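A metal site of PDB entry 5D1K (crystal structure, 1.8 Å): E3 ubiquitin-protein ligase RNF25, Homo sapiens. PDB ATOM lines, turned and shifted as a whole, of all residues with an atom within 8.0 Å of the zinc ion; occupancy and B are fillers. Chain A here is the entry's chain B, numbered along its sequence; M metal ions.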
ATOM      1  N   GLN A   9      22.454  16.271 -11.563  1.00  0.00           N
ATOM      2  CA  GLN A   9      21.528  16.353 -10.438  1.00  0.00           C
ATOM      3  C   GLN A   9      21.612  17.620  -9.597  1.00  0.00           C
ATOM      4  O   GLN A   9      22.696  18.158  -9.366  1.00  0.00           O
ATOM      5  CB  GLN A   9      21.695  15.121  -9.537  1.00  0.00           C
ATOM      6  CG  GLN A   9      21.863  15.456  -8.060  1.00  0.00           C
ATOM      7  CD  GLN A   9      22.918  14.607  -7.378  1.00  0.00           C
ATOM      8  OE1 GLN A   9      23.991  15.101  -7.033  1.00  0.00           O
ATOM      9  NE2 GLN A   9      22.612  13.331  -7.203  1.00  0.00           N
ATOM     10  N   CYS A  10      20.456  18.102  -9.146  1.00  0.00           N
ATOM     11  CA  CYS A  10      20.400  19.290  -8.308  1.00  0.00           C
ATOM     12  C   CYS A  10      21.052  18.879  -6.990  1.00  0.00           C
ATOM     13  O   CYS A  10      20.557  17.963  -6.326  1.00  0.00           O
ATOM     14  CB  CYS A  10      18.936  19.681  -8.067  1.00  0.00           C
ATOM     15  SG  CYS A  10      18.754  21.055  -6.922  1.00  0.00           S
ATOM     16  N   VAL A  11      22.169  19.481  -6.614  1.00  0.00           N
ATOM     17  CA  VAL A  11      22.876  18.977  -5.424  1.00  0.00           C
ATOM     18  C   VAL A  11      22.143  19.326  -4.126  1.00  0.00           C
ATOM     19  O   VAL A  11      22.494  18.831  -3.070  1.00  0.00           O
ATOM     20  CB  VAL A  11      24.369  19.451  -5.341  1.00  0.00           C
ATOM     21  CG1 VAL A  11      25.153  18.936  -6.532  1.00  0.00           C
ATOM     22  CG2 VAL A  11      24.473  20.969  -5.198  1.00  0.00           C
ATOM     23  N   ILE A  12      21.111  20.169  -4.209  1.00  0.00           N
ATOM     24  CA  ILE A  12      20.364  20.531  -3.017  1.00  0.00           C
ATOM     25  C   ILE A  12      19.373  19.437  -2.620  1.00  0.00           C
ATOM     26  O   ILE A  12      19.340  18.986  -1.463  1.00  0.00           O
ATOM     27  CB  ILE A  12      19.648  21.898  -3.172  1.00  0.00           C
ATOM     28  CG1 ILE A  12      20.688  23.013  -3.264  1.00  0.00           C
ATOM     29  CG2 ILE A  12      18.701  22.136  -2.022  1.00  0.00           C
ATOM     30  CD1 ILE A  12      20.119  24.365  -3.698  1.00  0.00           C
ATOM     31  N   CYS A  13      18.569  18.989  -3.573  1.00  0.00           N
ATOM     32  CA  CYS A  13      17.576  17.937  -3.292  1.00  0.00           C
ATOM     33  C   CYS A  13      18.055  16.522  -3.655  1.00  0.00           C
ATOM     34  O   CYS A  13      17.463  15.532  -3.218  1.00  0.00           O
ATOM     35  CB  CYS A  13      16.262  18.244  -4.016  1.00  0.00           C
ATOM     36  SG  CYS A  13      16.380  18.189  -5.832  1.00  0.00           S
ATOM     37  N   LEU A  14      19.100  16.442  -4.475  1.00  0.00           N
ATOM     38  CA  LEU A  14      19.656  15.173  -4.961  1.00  0.00           C
ATOM     39  C   LEU A  14      18.847  14.465  -6.056  1.00  0.00           C
ATOM     40  O   LEU A  14      19.138  13.315  -6.396  1.00  0.00           O
ATOM     41  CB  LEU A  14      19.960  14.202  -3.801  1.00  0.00           C
ATOM     42  CG  LEU A  14      20.991  14.733  -2.804  1.00  0.00           C
ATOM     43  CD1 LEU A  14      21.292  13.683  -1.735  1.00  0.00           C
ATOM     44  CD2 LEU A  14      22.254  15.157  -3.516  1.00  0.00           C
ATOM     45  N   TYR A  15      17.845  15.146  -6.590  1.00  0.00           N
ATOM     46  CA  TYR A  15      17.113  14.625  -7.748  1.00  0.00           C
ATOM     47  C   TYR A  15      17.629  15.272  -9.031  1.00  0.00           C
ATOM     48  O   TYR A  15      18.262  16.326  -9.003  1.00  0.00           O
ATOM     49  CB  TYR A  15      15.617  14.904  -7.613  1.00  0.00           C
ATOM     50  CG  TYR A  15      14.885  14.130  -6.534  1.00  0.00           C
ATOM     51  CD1 TYR A  15      15.024  14.460  -5.197  1.00  0.00           C
ATOM     52  CD2 TYR A  15      14.023  13.094  -6.878  1.00  0.00           C
ATOM     53  CE1 TYR A  15      14.340  13.761  -4.223  1.00  0.00           C
ATOM     54  CE2 TYR A  15      13.331  12.387  -5.894  1.00  0.00           C
ATOM     55  CZ  TYR A  15      13.501  12.725  -4.570  1.00  0.00           C
ATOM     56  OH  TYR A  15      12.808  12.036  -3.594  1.00  0.00           O
ATOM     57  N   GLY A  16      17.366  14.622 -10.157  1.00  0.00           N
ATOM     58  CA  GLY A  16      17.750  15.153 -11.455  1.00  0.00           C
ATOM     59  C   GLY A  16      16.693  16.090 -11.980  1.00  0.00           C
ATOM     60  O   GLY A  16      15.788  16.493 -11.250  1.00  0.00           O
ATOM     61  N   PHE A  17      16.787  16.453 -13.257  1.00  0.00           N
ATOM     62  CA  PHE A  17      15.861  17.428 -13.817  1.00  0.00           C
ATOM     63  C   PHE A  17      14.891  16.762 -14.801  1.00  0.00           C
ATOM     64  O   PHE A  17      15.281  15.872 -15.560  1.00  0.00           O
ATOM     65  CB  PHE A  17      16.644  18.581 -14.473  1.00  0.00           C
ATOM     66  CG  PHE A  17      17.565  19.291 -13.505  1.00  0.00           C
ATOM     67  CD1 PHE A  17      17.076  20.257 -12.644  1.00  0.00           C
ATOM     68  CD2 PHE A  17      18.913  18.966 -13.436  1.00  0.00           C
ATOM     69  CE1 PHE A  17      17.909  20.898 -11.736  1.00  0.00           C
ATOM     70  CE2 PHE A  17      19.748  19.609 -12.545  1.00  0.00           C
ATOM     71  CZ  PHE A  17      19.245  20.574 -11.686  1.00  0.00           C
ATOM     72  N   GLU A  21       9.834  20.445 -15.138  1.00  0.00           N
ATOM     73  CA  GLU A  21      10.287  21.127 -13.928  1.00  0.00           C
ATOM     74  C   GLU A  21      10.843  22.523 -14.192  1.00  0.00           C
ATOM     75  O   GLU A  21      11.432  22.783 -15.252  1.00  0.00           O
ATOM     76  CB  GLU A  21      11.359  20.290 -13.224  1.00  0.00           C
ATOM     77  CG  GLU A  21      10.817  19.107 -12.460  1.00  0.00           C
ATOM     78  CD  GLU A  21      11.916  18.189 -11.991  1.00  0.00           C
ATOM     79  OE1 GLU A  21      13.089  18.465 -12.310  1.00  0.00           O
ATOM     80  OE2 GLU A  21      11.611  17.189 -11.299  1.00  0.00           O
ATOM     81  N   ALA A  22      10.686  23.416 -13.213  1.00  0.00           N
ATOM     82  CA  ALA A  22      11.313  24.726 -13.252  1.00  0.00           C
ATOM     83  C   ALA A  22      12.673  24.662 -12.585  1.00  0.00           C
ATOM     84  O   ALA A  22      12.794  24.427 -11.375  1.00  0.00           O
ATOM     85  CB  ALA A  22      10.437  25.763 -12.576  1.00  0.00           C
ATOM     86  N   PHE A  23      13.723  24.852 -13.378  1.00  0.00           N
ATOM     87  CA  PHE A  23      15.080  24.870 -12.863  1.00  0.00           C
ATOM     88  C   PHE A  23      15.795  26.048 -13.482  1.00  0.00           C
ATOM     89  O   PHE A  23      15.302  26.654 -14.424  1.00  0.00           O
ATOM     90  CB  PHE A  23      15.811  23.560 -13.186  1.00  0.00           C
ATOM     91  CG  PHE A  23      15.790  23.177 -14.623  1.00  0.00           C
ATOM     92  CD1 PHE A  23      16.725  23.702 -15.514  1.00  0.00           C
ATOM     93  CD2 PHE A  23      14.858  22.268 -15.108  1.00  0.00           C
ATOM     94  CE1 PHE A  23      16.708  23.334 -16.853  1.00  0.00           C
ATOM     95  CE2 PHE A  23      14.832  21.911 -16.446  1.00  0.00           C
ATOM     96  CZ  PHE A  23      15.762  22.448 -17.312  1.00  0.00           C
ATOM     97  N   TYR A  31      23.344  24.010 -12.143  1.00  0.00           N
ATOM     98  CA  TYR A  31      21.889  23.947 -12.260  1.00  0.00           C
ATOM     99  C   TYR A  31      21.236  23.588 -10.936  1.00  0.00           C
ATOM    100  O   TYR A  31      21.717  22.694 -10.236  1.00  0.00           O
ATOM    101  CB  TYR A  31      21.485  22.888 -13.288  1.00  0.00           C
ATOM    102  CG  TYR A  31      21.792  23.255 -14.726  1.00  0.00           C
ATOM    103  CD1 TYR A  31      23.021  22.933 -15.292  1.00  0.00           C
ATOM    104  CD2 TYR A  31      20.849  23.902 -15.518  1.00  0.00           C
ATOM    105  CE1 TYR A  31      23.308  23.266 -16.615  1.00  0.00           C
ATOM    106  CE2 TYR A  31      21.136  24.235 -16.840  1.00  0.00           C
ATOM    107  CZ  TYR A  31      22.361  23.907 -17.373  1.00  0.00           C
ATOM    108  OH  TYR A  31      22.657  24.220 -18.692  1.00  0.00           O
ATOM    109  N   PHE A  32      20.126  24.266 -10.639  1.00  0.00           N
ATOM    110  CA  PHE A  32      19.340  23.961  -9.435  1.00  0.00           C
ATOM    111  C   PHE A  32      17.871  24.077  -9.776  1.00  0.00           C
ATOM    112  O   PHE A  32      17.508  24.850 -10.648  1.00  0.00           O
ATOM    113  CB  PHE A  32      19.662  24.946  -8.319  1.00  0.00           C
ATOM    114  CG  PHE A  32      21.129  25.040  -7.982  1.00  0.00           C
ATOM    115  CD1 PHE A  32      21.709  24.193  -7.041  1.00  0.00           C
ATOM    116  CD2 PHE A  32      21.927  26.001  -8.599  1.00  0.00           C
ATOM    117  CE1 PHE A  32      23.050  24.295  -6.737  1.00  0.00           C
ATOM    118  CE2 PHE A  32      23.274  26.108  -8.288  1.00  0.00           C
ATOM    119  CZ  PHE A  32      23.835  25.255  -7.357  1.00  0.00           C
ATOM    120  N   HIS A  33      17.004  23.348  -9.085  1.00  0.00           N
ATOM    121  CA  HIS A  33      15.586  23.628  -9.212  1.00  0.00           C
ATOM    122  C   HIS A  33      15.389  25.004  -8.630  1.00  0.00           C
ATOM    123  O   HIS A  33      16.088  25.393  -7.690  1.00  0.00           O
ATOM    124  CB  HIS A  33      14.719  22.601  -8.467  1.00  0.00           C
ATOM    125  CG  HIS A  33      14.811  21.210  -9.018  1.00  0.00           C
ATOM    126  ND1 HIS A  33      15.565  20.211  -8.437  1.00  0.00           N
ATOM    127  CD2 HIS A  33      14.249  20.661 -10.123  1.00  0.00           C
ATOM    128  CE1 HIS A  33      15.473  19.113  -9.160  1.00  0.00           C
ATOM    129  NE2 HIS A  33      14.669  19.359 -10.178  1.00  0.00           N
ATOM    130  N   CYS A  34      14.472  25.775  -9.196  1.00  0.00           N
ATOM    131  CA  CYS A  34      14.265  27.120  -8.698  1.00  0.00           C
ATOM    132  C   CYS A  34      13.865  27.106  -7.233  1.00  0.00           C
ATOM    133  O   CYS A  34      14.287  27.949  -6.442  1.00  0.00           O
ATOM    134  CB  CYS A  34      13.196  27.821  -9.521  1.00  0.00           C
ATOM    135  SG  CYS A  34      13.790  28.076 -11.208  1.00  0.00           S
ATOM    136  N   HIS A  35      13.009  26.146  -6.901  1.00  0.00           N
ATOM    137  CA  HIS A  35      12.476  26.021  -5.549  1.00  0.00           C
ATOM    138  C   HIS A  35      13.610  25.729  -4.562  1.00  0.00           C
ATOM    139  O   HIS A  35      13.678  26.322  -3.477  1.00  0.00           O
ATOM    140  CB  HIS A  35      11.437  24.903  -5.511  1.00  0.00           C
ATOM    141  CG  HIS A  35      11.010  24.524  -4.127  1.00  0.00           C
ATOM    142  ND1 HIS A  35      10.020  25.209  -3.446  1.00  0.00           N
ATOM    143  CD2 HIS A  35      11.427  23.532  -3.299  1.00  0.00           C
ATOM    144  CE1 HIS A  35       9.852  24.654  -2.255  1.00  0.00           C
ATOM    145  NE2 HIS A  35      10.695  23.643  -2.144  1.00  0.00           N
ATOM    146  N   CYS A  36      14.481  24.804  -4.940  1.00  0.00           N
ATOM    147  CA  CYS A  36      15.622  24.428  -4.103  1.00  0.00           C
ATOM    148  C   CYS A  36      16.559  25.606  -3.866  1.00  0.00           C
ATOM    149  O   CYS A  36      16.990  25.854  -2.742  1.00  0.00           O
ATOM    150  CB  CYS A  36      16.387  23.269  -4.738  1.00  0.00           C
ATOM    151  SG  CYS A  36      15.408  21.758  -4.940  1.00  0.00           S
ATOM    152  N   LEU A  37      16.904  26.309  -4.943  1.00  0.00           N
ATOM    153  CA  LEU A  37      17.801  27.446  -4.830  1.00  0.00           C
ATOM    154  C   LEU A  37      17.164  28.579  -4.018  1.00  0.00           C
ATOM    155  O   LEU A  37      17.849  29.255  -3.264  1.00  0.00           O
ATOM    156  CB  LEU A  37      18.240  27.937  -6.216  1.00  0.00           C
ATOM    157  CG  LEU A  37      19.377  28.976  -6.203  1.00  0.00           C
ATOM    158  CD1 LEU A  37      20.641  28.369  -5.604  1.00  0.00           C
ATOM    159  CD2 LEU A  37      19.652  29.524  -7.606  1.00  0.00           C
ATOM    160  N   PRO A  93       9.170  21.197  -7.586  1.00  0.00           N
ATOM    161  CA  PRO A  93       9.230  19.941  -8.335  1.00  0.00           C
ATOM    162  C   PRO A  93       8.467  18.837  -7.627  1.00  0.00           C
ATOM    163  O   PRO A  93       8.445  18.813  -6.398  1.00  0.00           O
ATOM    164  CB  PRO A  93      10.727  19.597  -8.327  1.00  0.00           C
ATOM    165  CG  PRO A  93      11.421  20.818  -7.877  1.00  0.00           C
ATOM    166  CD  PRO A  93      10.473  21.561  -7.015  1.00  0.00           C
ATOM    167  N   GLN A  95       8.458  15.177  -6.646  1.00  0.00           N
ATOM    168  CA  GLN A  95       9.458  14.140  -6.542  1.00  0.00           C
ATOM    169  C   GLN A  95       9.041  13.097  -5.512  1.00  0.00           C
ATOM    170  O   GLN A  95       8.962  13.396  -4.321  1.00  0.00           O
ATOM    171  CB  GLN A  95      10.794  14.765  -6.151  1.00  0.00           C
ATOM    172  CG  GLN A  95      11.082  16.066  -6.886  1.00  0.00           C
ATOM    173  CD  GLN A  95      12.243  16.846  -6.312  1.00  0.00           C
ATOM    174  OE1 GLN A  95      12.248  17.224  -5.132  1.00  0.00           O
ATOM    175  NE2 GLN A  95      13.230  17.114  -7.142  1.00  0.00           N
HETATM  176 ZN    ZN M   1      16.550  20.400  -6.402  1.00  0.00          ZN
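NE2 of His 33 lies within hydrogen-bond range of OE1 of Glu 21 (2.8 Å). The side-chain sulfur (SG) of Cys 10 sits close to the backbone NH (N) of Ile 12, at 3.7 Å. NE2 of His 33 lies within hydrogen-bond range of O of Gly 16 (3.3 Å). The side-chain sulfur (SG) of Cys 13 lies close to the side-chain amide nitrogen (NE2) of Gln 95. The backbone NH (N) of Cys 10 is in hydrogen-bond range of the backbone carbonyl oxygen (O) of Tyr 15 (2.8 Å). The backbone NH of Tyr 15 lies close to the side-chain sulfur of Cys 13.
Of the 21 residues printed, 4 come within 4 Å of the zinc ion.
The zinc ion is bound by ND1 of His 33, SG of Cys 13, SG of Cys 36 and SG of Cys 10. The zinc ion has four donor atoms within binding distance.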
